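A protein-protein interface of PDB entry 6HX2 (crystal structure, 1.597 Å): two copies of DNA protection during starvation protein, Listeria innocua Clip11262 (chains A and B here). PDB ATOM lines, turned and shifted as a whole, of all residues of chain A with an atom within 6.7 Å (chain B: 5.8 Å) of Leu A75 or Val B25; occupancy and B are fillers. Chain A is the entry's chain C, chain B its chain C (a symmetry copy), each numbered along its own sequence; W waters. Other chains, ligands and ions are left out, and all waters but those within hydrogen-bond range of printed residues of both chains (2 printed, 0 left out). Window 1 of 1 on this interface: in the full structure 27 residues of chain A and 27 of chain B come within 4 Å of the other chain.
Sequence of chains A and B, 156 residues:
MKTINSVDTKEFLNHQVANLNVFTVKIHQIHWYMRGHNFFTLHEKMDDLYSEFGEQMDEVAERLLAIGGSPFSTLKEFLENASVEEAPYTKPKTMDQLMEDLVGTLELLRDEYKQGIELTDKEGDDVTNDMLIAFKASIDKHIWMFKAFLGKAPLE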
ATOM      1  N   ASN A  21       5.945 -16.636   7.767  1.00  0.00           N
ATOM      2  CA  ASN A  21       7.071 -16.545   8.693  1.00  0.00           C
ATOM      3  C   ASN A  21       7.262 -15.126   9.216  1.00  0.00           C
ATOM      4  O   ASN A  21       7.639 -14.936  10.381  1.00  0.00           O
ATOM      5  CB  ASN A  21       8.349 -17.043   8.019  1.00  0.00           C
ATOM      6  CG  ASN A  21       8.497 -18.543   8.113  1.00  0.00           C
ATOM      7  OD1 ASN A  21       9.017 -19.061   9.102  1.00  0.00           O
ATOM      8  ND2 ASN A  21       8.051 -19.251   7.082  1.00  0.00           N
ATOM      9  N   PHE A  72      10.876 -21.801   0.281  1.00  0.00           N
ATOM     10  CA  PHE A  72      11.836 -20.940   0.959  1.00  0.00           C
ATOM     11  C   PHE A  72      12.051 -21.449   2.379  1.00  0.00           C
ATOM     12  O   PHE A  72      11.113 -21.897   3.044  1.00  0.00           O
ATOM     13  CB  PHE A  72      11.323 -19.498   1.013  1.00  0.00           C
ATOM     14  CG  PHE A  72      11.104 -18.867  -0.335  1.00  0.00           C
ATOM     15  CD1 PHE A  72      12.078 -18.924  -1.308  1.00  0.00           C
ATOM     16  CD2 PHE A  72       9.924 -18.196  -0.614  1.00  0.00           C
ATOM     17  CE1 PHE A  72      11.887 -18.337  -2.549  1.00  0.00           C
ATOM     18  CE2 PHE A  72       9.720 -17.603  -1.857  1.00  0.00           C
ATOM     19  CZ  PHE A  72      10.698 -17.673  -2.823  1.00  0.00           C
ATOM     20  N   SER A  73      13.303 -21.381   2.861  1.00  0.00           N
ATOM     21  CA  SER A  73      13.589 -22.006   4.152  1.00  0.00           C
ATOM     22  C   SER A  73      14.731 -21.325   4.890  1.00  0.00           C
ATOM     23  O   SER A  73      15.478 -21.990   5.619  1.00  0.00           O
ATOM     24  CB  SER A  73      13.906 -23.491   3.966  1.00  0.00           C
ATOM     25  OG  SER A  73      15.065 -23.662   3.175  1.00  0.00           O
ATOM     26  N   THR A  74      14.876 -20.015   4.708  1.00  0.00           N
ATOM     27  CA  THR A  74      15.847 -19.183   5.404  1.00  0.00           C
ATOM     28  C   THR A  74      15.185 -17.835   5.663  1.00  0.00           C
ATOM     29  O   THR A  74      14.276 -17.427   4.929  1.00  0.00           O
ATOM     30  CB  THR A  74      17.129 -18.958   4.585  1.00  0.00           C
ATOM     31  OG1 THR A  74      16.810 -18.297   3.339  1.00  0.00           O
ATOM     32  CG2 THR A  74      17.846 -20.294   4.296  1.00  0.00           C
ATOM     33  N   LEU A  75      15.648 -17.139   6.703  1.00  0.00           N
ATOM     34  CA  LEU A  75      15.126 -15.802   6.969  1.00  0.00           C
ATOM     35  C   LEU A  75      15.414 -14.875   5.797  1.00  0.00           C
ATOM     36  O   LEU A  75      14.582 -14.033   5.441  1.00  0.00           O
ATOM     37  CB  LEU A  75      15.732 -15.241   8.256  1.00  0.00           C
ATOM     38  CG  LEU A  75      15.183 -15.724   9.598  1.00  0.00           C
ATOM     39  CD1 LEU A  75      15.554 -17.184   9.898  1.00  0.00           C
ATOM     40  CD2 LEU A  75      15.705 -14.805  10.701  1.00  0.00           C
ATOM     41  N   LYS A  76      16.592 -15.016   5.190  1.00  0.00           N
ATOM     42  CA  LYS A  76      16.951 -14.172   4.057  1.00  0.00           C
ATOM     43  C   LYS A  76      15.922 -14.304   2.942  1.00  0.00           C
ATOM     44  O   LYS A  76      15.472 -13.305   2.371  1.00  0.00           O
ATOM     45  CB  LYS A  76      18.352 -14.547   3.565  1.00  0.00           C
ATOM     46  CG  LYS A  76      18.872 -13.724   2.387  1.00  0.00           C
ATOM     47  CD  LYS A  76      20.318 -14.091   2.077  1.00  0.00           C
ATOM     48  CE  LYS A  76      20.868 -13.344   0.852  1.00  0.00           C
ATOM     49  NZ  LYS A  76      20.288 -13.823  -0.421  1.00  0.00           N
ATOM     50  N   GLU A  77      15.531 -15.536   2.620  1.00  0.00           N
ATOM     51  CA  GLU A  77      14.538 -15.731   1.570  1.00  0.00           C
ATOM     52  C   GLU A  77      13.179 -15.178   1.982  1.00  0.00           C
ATOM     53  O   GLU A  77      12.474 -14.588   1.158  1.00  0.00           O
ATOM     54  CB  GLU A  77      14.433 -17.211   1.218  1.00  0.00           C
ATOM     55  CG  GLU A  77      15.645 -17.756   0.474  1.00  0.00           C
ATOM     56  CD  GLU A  77      15.571 -19.260   0.329  1.00  0.00           C
ATOM     57  OE1 GLU A  77      15.560 -19.956   1.368  1.00  0.00           O
ATOM     58  OE2 GLU A  77      15.500 -19.745  -0.817  1.00  0.00           O
ATOM     59  N   PHE A  78      12.790 -15.354   3.248  1.00  0.00           N
ATOM     60  CA  PHE A  78      11.501 -14.824   3.686  1.00  0.00           C
ATOM     61  C   PHE A  78      11.459 -13.312   3.506  1.00  0.00           C
ATOM     62  O   PHE A  78      10.480 -12.763   2.990  1.00  0.00           O
ATOM     63  CB  PHE A  78      11.223 -15.179   5.145  1.00  0.00           C
ATOM     64  CG  PHE A  78      11.234 -16.648   5.454  1.00  0.00           C
ATOM     65  CD1 PHE A  78      10.941 -17.606   4.490  1.00  0.00           C
ATOM     66  CD2 PHE A  78      11.544 -17.065   6.742  1.00  0.00           C
ATOM     67  CE1 PHE A  78      10.964 -18.955   4.807  1.00  0.00           C
ATOM     68  CE2 PHE A  78      11.575 -18.411   7.078  1.00  0.00           C
ATOM     69  CZ  PHE A  78      11.286 -19.370   6.117  1.00  0.00           C
ATOM     70  N   LEU A  79      12.526 -12.616   3.925  1.00  0.00           N
ATOM     71  CA  LEU A  79      12.546 -11.160   3.792  1.00  0.00           C
ATOM     72  C   LEU A  79      12.600 -10.726   2.334  1.00  0.00           C
ATOM     73  O   LEU A  79      12.036  -9.686   1.982  1.00  0.00           O
ATOM     74  CB  LEU A  79      13.725 -10.570   4.563  1.00  0.00           C
ATOM     75  CG  LEU A  79      13.533 -10.409   6.066  1.00  0.00           C
ATOM     76  CD1 LEU A  79      14.802  -9.851   6.698  1.00  0.00           C
ATOM     77  CD2 LEU A  79      12.356  -9.492   6.381  1.00  0.00           C
ATOM     78  N   GLU A  80      13.255 -11.508   1.471  1.00  0.00           N
ATOM     79  CA  GLU A  80      13.336 -11.158   0.059  1.00  0.00           C
ATOM     80  C   GLU A  80      11.988 -11.264  -0.636  1.00  0.00           C
ATOM     81  O   GLU A  80      11.792 -10.623  -1.674  1.00  0.00           O
ATOM     82  CB  GLU A  80      14.333 -12.069  -0.659  1.00  0.00           C
ATOM     83  CG  GLU A  80      15.791 -11.737  -0.401  1.00  0.00           C
ATOM     84  CD  GLU A  80      16.748 -12.807  -0.929  1.00  0.00           C
ATOM     85  OE1 GLU A  80      16.285 -13.927  -1.273  1.00  0.00           O
ATOM     86  OE2 GLU A  80      17.967 -12.528  -0.981  1.00  0.00           O
ATOM     87  N   LEU B  20      18.089 -18.448  18.140  1.00  0.00           N
ATOM     88  CA  LEU B  20      17.068 -19.487  18.221  1.00  0.00           C
ATOM     89  C   LEU B  20      16.039 -19.332  17.119  1.00  0.00           C
ATOM     90  O   LEU B  20      15.484 -20.332  16.651  1.00  0.00           O
ATOM     91  CB  LEU B  20      16.406 -19.470  19.601  1.00  0.00           C
ATOM     92  CG  LEU B  20      17.330 -19.983  20.703  1.00  0.00           C
ATOM     93  CD1 LEU B  20      16.821 -19.571  22.109  1.00  0.00           C
ATOM     94  CD2 LEU B  20      17.425 -21.507  20.593  1.00  0.00           C
ATOM     95  N   ASN B  21      15.784 -18.103  16.675  1.00  0.00           N
ATOM     96  CA  ASN B  21      14.901 -17.925  15.526  1.00  0.00           C
ATOM     97  C   ASN B  21      15.541 -18.424  14.236  1.00  0.00           C
ATOM     98  O   ASN B  21      14.848 -18.964  13.364  1.00  0.00           O
ATOM     99  CB  ASN B  21      14.499 -16.458  15.392  1.00  0.00           C
ATOM    100  CG  ASN B  21      13.311 -16.108  16.257  1.00  0.00           C
ATOM    101  OD1 ASN B  21      12.163 -16.286  15.847  1.00  0.00           O
ATOM    102  ND2 ASN B  21      13.575 -15.602  17.456  1.00  0.00           N
ATOM    103  N   VAL B  22      16.851 -18.229  14.070  1.00  0.00           N
ATOM    104  CA  VAL B  22      17.516 -18.785  12.897  1.00  0.00           C
ATOM    105  C   VAL B  22      17.514 -20.304  12.973  1.00  0.00           C
ATOM    106  O   VAL B  22      17.310 -20.994  11.960  1.00  0.00           O
ATOM    107  CB  VAL B  22      18.941 -18.214  12.760  1.00  0.00           C
ATOM    108  CG1 VAL B  22      19.678 -18.835  11.550  1.00  0.00           C
ATOM    109  CG2 VAL B  22      18.884 -16.704  12.604  1.00  0.00           C
ATOM    110  N   PHE B  23      17.720 -20.848  14.176  1.00  0.00           N
ATOM    111  CA  PHE B  23      17.792 -22.295  14.356  1.00  0.00           C
ATOM    112  C   PHE B  23      16.448 -22.962  14.072  1.00  0.00           C
ATOM    113  O   PHE B  23      16.403 -24.009  13.420  1.00  0.00           O
ATOM    114  CB  PHE B  23      18.239 -22.617  15.777  1.00  0.00           C
ATOM    115  CG  PHE B  23      18.498 -24.074  16.032  1.00  0.00           C
ATOM    116  CD1 PHE B  23      19.021 -24.901  15.050  1.00  0.00           C
ATOM    117  CD2 PHE B  23      18.222 -24.616  17.280  1.00  0.00           C
ATOM    118  CE1 PHE B  23      19.277 -26.249  15.315  1.00  0.00           C
ATOM    119  CE2 PHE B  23      18.462 -25.958  17.544  1.00  0.00           C
ATOM    120  CZ  PHE B  23      18.985 -26.772  16.566  1.00  0.00           C
ATOM    121  N   THR B  24      15.340 -22.393  14.559  1.00  0.00           N
ATOM    122  CA  THR B  24      14.057 -23.053  14.323  1.00  0.00           C
ATOM    123  C   THR B  24      13.705 -23.049  12.839  1.00  0.00           C
ATOM    124  O   THR B  24      13.125 -24.018  12.334  1.00  0.00           O
ATOM    125  CB  THR B  24      12.933 -22.410  15.145  1.00  0.00           C
ATOM    126  OG1 THR B  24      12.855 -21.005  14.880  1.00  0.00           O
ATOM    127  CG2 THR B  24      13.139 -22.673  16.646  1.00  0.00           C
ATOM    128  N   VAL B  25      14.064 -21.987  12.117  1.00  0.00           N
ATOM    129  CA  VAL B  25      13.844 -21.992  10.673  1.00  0.00           C
ATOM    130  C   VAL B  25      14.715 -23.054  10.006  1.00  0.00           C
ATOM    131  O   VAL B  25      14.270 -23.738   9.078  1.00  0.00           O
ATOM    132  CB  VAL B  25      14.086 -20.593  10.086  1.00  0.00           C
ATOM    133  CG1 VAL B  25      14.083 -20.641   8.555  1.00  0.00           C
ATOM    134  CG2 VAL B  25      13.017 -19.640  10.600  1.00  0.00           C
ATOM    135  N   LYS B  26      15.956 -23.222  10.475  1.00  0.00           N
ATOM    136  CA  LYS B  26      16.815 -24.290   9.959  1.00  0.00           C
ATOM    137  C   LYS B  26      16.217 -25.665  10.235  1.00  0.00           C
ATOM    138  O   LYS B  26      16.308 -26.571   9.397  1.00  0.00           O
ATOM    139  CB  LYS B  26      18.212 -24.200  10.580  1.00  0.00           C
ATOM    140  CG  LYS B  26      19.177 -25.276  10.084  1.00  0.00           C
ATOM    141  CD  LYS B  26      20.502 -25.280  10.848  1.00  0.00           C
ATOM    142  CE  LYS B  26      21.340 -24.046  10.576  1.00  0.00           C
ATOM    143  NZ  LYS B  26      21.803 -24.011   9.150  1.00  0.00           N
ATOM    144  N   ILE B  27      15.625 -25.851  11.418  1.00  0.00           N
ATOM    145  CA  ILE B  27      14.984 -27.124  11.734  1.00  0.00           C
ATOM    146  C   ILE B  27      13.887 -27.414  10.731  1.00  0.00           C
ATOM    147  O   ILE B  27      13.726 -28.557  10.281  1.00  0.00           O
ATOM    148  CB  ILE B  27      14.462 -27.106  13.181  1.00  0.00           C
ATOM    149  CG1 ILE B  27      15.665 -27.125  14.143  1.00  0.00           C
ATOM    150  CG2 ILE B  27      13.481 -28.248  13.449  1.00  0.00           C
ATOM    151  CD1 ILE B  27      15.338 -26.776  15.571  1.00  0.00           C
ATOM    152  N   HIS B  28      13.116 -26.387  10.366  1.00  0.00           N
ATOM    153  CA  HIS B  28      12.088 -26.561   9.345  1.00  0.00           C
ATOM    154  C   HIS B  28      12.690 -26.902   7.992  1.00  0.00           C
ATOM    155  O   HIS B  28      12.157 -27.757   7.280  1.00  0.00           O
ATOM    156  CB  HIS B  28      11.227 -25.311   9.237  1.00  0.00           C
ATOM    157  CG  HIS B  28       9.963 -25.384  10.027  1.00  0.00           C
ATOM    158  ND1 HIS B  28       9.148 -24.292  10.228  1.00  0.00           N
ATOM    159  CD2 HIS B  28       9.349 -26.429  10.635  1.00  0.00           C
ATOM    160  CE1 HIS B  28       8.098 -24.657  10.942  1.00  0.00           C
ATOM    161  NE2 HIS B  28       8.199 -25.948  11.203  1.00  0.00           N
ATOM    162  N   GLN B  29      13.785 -26.247   7.616  1.00  0.00           N
ATOM    163  CA  GLN B  29      14.457 -26.591   6.369  1.00  0.00           C
ATOM    164  C   GLN B  29      14.781 -28.080   6.316  1.00  0.00           C
ATOM    165  O   GLN B  29      14.542 -28.752   5.303  1.00  0.00           O
ATOM    166  CB  GLN B  29      15.733 -25.770   6.226  1.00  0.00           C
ATOM    167  CG  GLN B  29      16.541 -26.114   4.994  1.00  0.00           C
ATOM    168  CD  GLN B  29      17.789 -25.264   4.894  1.00  0.00           C
ATOM    169  OE1 GLN B  29      18.863 -25.642   5.389  1.00  0.00           O
ATOM    170  NE2 GLN B  29      17.650 -24.091   4.306  1.00  0.00           N
ATOM    171  N   ILE B  30      15.334 -28.609   7.407  1.00  0.00           N
ATOM    172  CA  ILE B  30      15.688 -30.025   7.473  1.00  0.00           C
ATOM    173  C   ILE B  30      14.435 -30.902   7.421  1.00  0.00           C
ATOM    174  O   ILE B  30      14.384 -31.893   6.672  1.00  0.00           O
ATOM    175  CB  ILE B  30      16.530 -30.273   8.740  1.00  0.00           C
ATOM    176  CG1 ILE B  30      17.858 -29.522   8.593  1.00  0.00           C
ATOM    177  CG2 ILE B  30      16.749 -31.742   8.969  1.00  0.00           C
ATOM    178  CD1 ILE B  30      18.655 -29.397   9.873  1.00  0.00           C
ATOM    179  N   TRP B  32      11.570 -30.279   6.067  1.00  0.00           N
ATOM    180  CA  TRP B  32      10.905 -30.258   4.765  1.00  0.00           C
ATOM    181  C   TRP B  32      11.693 -30.996   3.684  1.00  0.00           C
ATOM    182  O   TRP B  32      11.102 -31.702   2.863  1.00  0.00           O
ATOM    183  CB  TRP B  32      10.682 -28.815   4.328  1.00  0.00           C
ATOM    184  CG  TRP B  32       9.659 -28.071   5.132  1.00  0.00           C
ATOM    185  CD1 TRP B  32       8.597 -28.596   5.798  1.00  0.00           C
ATOM    186  CD2 TRP B  32       9.620 -26.656   5.364  1.00  0.00           C
ATOM    187  NE1 TRP B  32       7.878 -27.594   6.421  1.00  0.00           N
ATOM    188  CE2 TRP B  32       8.503 -26.396   6.187  1.00  0.00           C
ATOM    189  CE3 TRP B  32      10.425 -25.587   4.961  1.00  0.00           C
ATOM    190  CZ2 TRP B  32       8.164 -25.110   6.601  1.00  0.00           C
ATOM    191  CZ3 TRP B  32      10.091 -24.306   5.380  1.00  0.00           C
ATOM    192  CH2 TRP B  32       8.977 -24.079   6.194  1.00  0.00           C
ATOM    193  N   TYR B  50      11.633 -28.469  16.821  1.00  0.00           N
ATOM    194  CA  TYR B  50      11.050 -27.174  16.501  1.00  0.00           C
ATOM    195  C   TYR B  50      10.256 -26.638  17.689  1.00  0.00           C
ATOM    196  O   TYR B  50      10.390 -25.468  18.071  1.00  0.00           O
ATOM    197  CB  TYR B  50      10.165 -27.298  15.256  1.00  0.00           C
ATOM    198  CG  TYR B  50       9.664 -25.961  14.768  1.00  0.00           C
ATOM    199  CD1 TYR B  50      10.436 -25.189  13.908  1.00  0.00           C
ATOM    200  CD2 TYR B  50       8.437 -25.459  15.183  1.00  0.00           C
ATOM    201  CE1 TYR B  50      10.003 -23.951  13.471  1.00  0.00           C
ATOM    202  CE2 TYR B  50       7.985 -24.218  14.744  1.00  0.00           C
ATOM    203  CZ  TYR B  50       8.783 -23.467  13.894  1.00  0.00           C
ATOM    204  OH  TYR B  50       8.363 -22.239  13.451  1.00  0.00           O
ATOM    205  N   THR B  74      12.062  -8.957  14.932  1.00  0.00           N
ATOM    206  CA  THR B  74      11.905  -8.890  13.485  1.00  0.00           C
ATOM    207  C   THR B  74      12.951  -9.811  12.872  1.00  0.00           C
ATOM    208  O   THR B  74      14.003 -10.062  13.474  1.00  0.00           O
ATOM    209  CB  THR B  74      12.109  -7.469  12.933  1.00  0.00           C
ATOM    210  OG1 THR B  74      13.443  -7.006  13.243  1.00  0.00           O
ATOM    211  CG2 THR B  74      11.070  -6.490  13.520  1.00  0.00           C
ATOM    212  N   LEU B  75      12.667 -10.310  11.667  1.00  0.00           N
ATOM    213  CA  LEU B  75      13.652 -11.134  10.974  1.00  0.00           C
ATOM    214  C   LEU B  75      14.921 -10.337  10.710  1.00  0.00           C
ATOM    215  O   LEU B  75      16.032 -10.871  10.810  1.00  0.00           O
ATOM    216  CB  LEU B  75      13.072 -11.666   9.663  1.00  0.00           C
ATOM    217  CG  LEU B  75      12.112 -12.854   9.713  1.00  0.00           C
ATOM    218  CD1 LEU B  75      10.751 -12.489  10.325  1.00  0.00           C
ATOM    219  CD2 LEU B  75      11.929 -13.397   8.297  1.00  0.00           C
ATOM    220  N   PHE B  78      17.022 -10.437  13.741  1.00  0.00           N
ATOM    221  CA  PHE B  78      17.592 -11.763  13.966  1.00  0.00           C
ATOM    222  C   PHE B  78      18.803 -11.981  13.068  1.00  0.00           C
ATOM    223  O   PHE B  78      19.850 -12.455  13.522  1.00  0.00           O
ATOM    224  CB  PHE B  78      16.559 -12.860  13.717  1.00  0.00           C
ATOM    225  CG  PHE B  78      15.312 -12.758  14.546  1.00  0.00           C
ATOM    226  CD1 PHE B  78      15.303 -12.135  15.789  1.00  0.00           C
ATOM    227  CD2 PHE B  78      14.131 -13.305  14.062  1.00  0.00           C
ATOM    228  CE1 PHE B  78      14.134 -12.055  16.529  1.00  0.00           C
ATOM    229  CE2 PHE B  78      12.950 -13.232  14.786  1.00  0.00           C
ATOM    230  CZ  PHE B  78      12.938 -12.608  16.026  1.00  0.00           C
ATOM    231  N   LEU B  79      18.679 -11.632  11.779  1.00  0.00           N
ATOM    232  CA  LEU B  79      19.801 -11.825  10.860  1.00  0.00           C
ATOM    233  C   LEU B  79      20.968 -10.907  11.192  1.00  0.00           C
ATOM    234  O   LEU B  79      22.125 -11.291  10.997  1.00  0.00           O
ATOM    235  CB  LEU B  79      19.351 -11.608   9.417  1.00  0.00           C
ATOM    236  CG  LEU B  79      18.633 -12.777   8.753  1.00  0.00           C
ATOM    237  CD1 LEU B  79      18.212 -12.396   7.340  1.00  0.00           C
ATOM    238  CD2 LEU B  79      19.515 -14.020   8.710  1.00  0.00           C
ATOM    239  N   GLU B  86      22.814 -19.778   8.287  1.00  0.00           N
ATOM    240  CA  GLU B  86      21.779 -20.385   7.460  1.00  0.00           C
ATOM    241  C   GLU B  86      22.220 -20.288   6.009  1.00  0.00           C
ATOM    242  O   GLU B  86      23.012 -19.417   5.628  1.00  0.00           O
ATOM    243  CB  GLU B  86      20.399 -19.710   7.638  1.00  0.00           C
ATOM    244  CG  GLU B  86      20.410 -18.207   7.337  1.00  0.00           C
ATOM    245  CD  GLU B  86      19.017 -17.596   7.215  1.00  0.00           C
ATOM    246  OE1 GLU B  86      18.056 -18.133   7.826  1.00  0.00           O
ATOM    247  OE2 GLU B  86      18.898 -16.571   6.496  1.00  0.00           O
HETATM  248  O   HOH W   1      10.059 -21.722   9.615  1.00  0.00           O
HETATM  249  O   HOH W   2      17.595 -22.426   7.350  1.00  0.00           O
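The backbone NH (N) of Leu A75 is in hydrogen-bond range of the side-chain carboxylate (OE1) of Glu B86 (2.8 Å). The backbone NH (N) of Lys A76 lies within hydrogen-bond range of the side-chain carboxylate (OE2) of Glu B86. OG of Ser A73 sits at hydrogen-bond distance from NE2 of Gln B29 (2.9 Å).
The side-chain hydroxyl of Thr A74 is in hydrogen-bond range of the side-chain carboxylate of Glu A77. N of Ser A73 lies within hydrogen-bond range of OE1 of Glu A77 (3.1 Å). OE2 of Glu A80 is in salt-bridge range of NZ of Lys A76 (2.7 Å). The side-chain hydroxyl of Thr B24 is in hydrogen-bond range of the backbone carbonyl oxygen of Asn B21 (3.2 Å).
Among the printed residues, pairs that only touch across the chains: Asn A21 with Leu B75, Phe A72 with Trp B32, Ser A73 with Val B25, Thr A74 with Val B25, Thr A74 with Gln B29, Thr A74 with Glu B86, Leu A75 with Asn B21, Leu A75 with Val B22, Leu A75 with Val B25, Leu A75 with Leu B75, Leu A75 with Phe B78, Leu A75 with Leu B79, Lys A76 with Leu B79, Phe A78 with Val B25, Phe A78 with Leu B75 and Leu A79 with Leu B75.
Of the printed residues of chain B, Leu A75 touches Asn B21, Val B22, Val B25, Leu B75, Phe B78, Leu B79 and Glu B86. Of the printed residues of chain B, Lys A76 touches Leu B79 (3.8 Å) and Glu B86 (3.1 Å). Printed residues of chain B within 4 Å of Phe A78: Val B25 and Leu B75. Of the printed residues of chain A, Val B25 touches Ser A73, Thr A74, Leu A75 and Phe A78. Ile B27 touches none of the printed residues of chain A. Thr B74 touches none of the printed residues of chain A. Of the printed residues of chain A, Leu B79 touches Leu A75 (3.8 Å) and Lys A76 (3.8 Å). The nearest printed residue of chain A that does not touch Val B25 is Asn A21 (4.3 Å). The nearest printed residue of chain A that does not touch Asn B21 is Phe A78 (7.1 Å).
Of the 18 printed residues of chain B, 9 touch a printed residue of chain A. Printed residues of chain B that touch a printed residue of chain A: Asn B21, Val B22, Val B25, Gln B29, Trp B32, Leu B75, Phe B78, Leu B79 and Glu B86. Hydrophobic or aromatic side chains of chain B within 4 Å of the printed part of chain A: Val B25, Trp B32, Leu B75, Phe B78 and Leu B79. Of the 10 printed residues of chain A, 8 touch a printed residue of chain B. Printed residues of chain A that touch a printed residue of chain B: Asn A21, Phe A72, Ser A73, Thr A74, Leu A75, Lys A76, Phe A78 and Leu A79. Hydrophobic or aromatic side chains of chain A within 4 Å of the printed part of chain B: Leu A75, Phe A78 and Leu A79. Among the printed residues, 19 pairs touch across the chains. Among the printed residues, no Asp or Glu carboxylate lies within 4 Å of a Lys or Arg side-chain nitrogen of the other chain.
Asn A21 touches Leu B75, and with the chains exchanged Leu A75 touches Asn B21. Leu B75 touches its own counterpart, Leu A75. Leu A75 touches Phe B78, and with the chains exchanged Phe A78 touches Leu B75. Leu A75 touches Leu B79, and with the chains exchanged Leu A79 touches Leu B75. 5 positions are printed for both chains. Of the 19 pairs that touch across the chains among the printed residues, 7 have their exchanged pair printed and touching as well.
Water W2 bridges the backbone carbonyl oxygen (O) of Ser A73 and the side-chain amide nitrogen (NE2) of Gln B29. Water W1 lies within hydrogen-bond range of a ring nitrogen (ND1) of His B28 and the side-chain amide oxygen of Asn A21.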
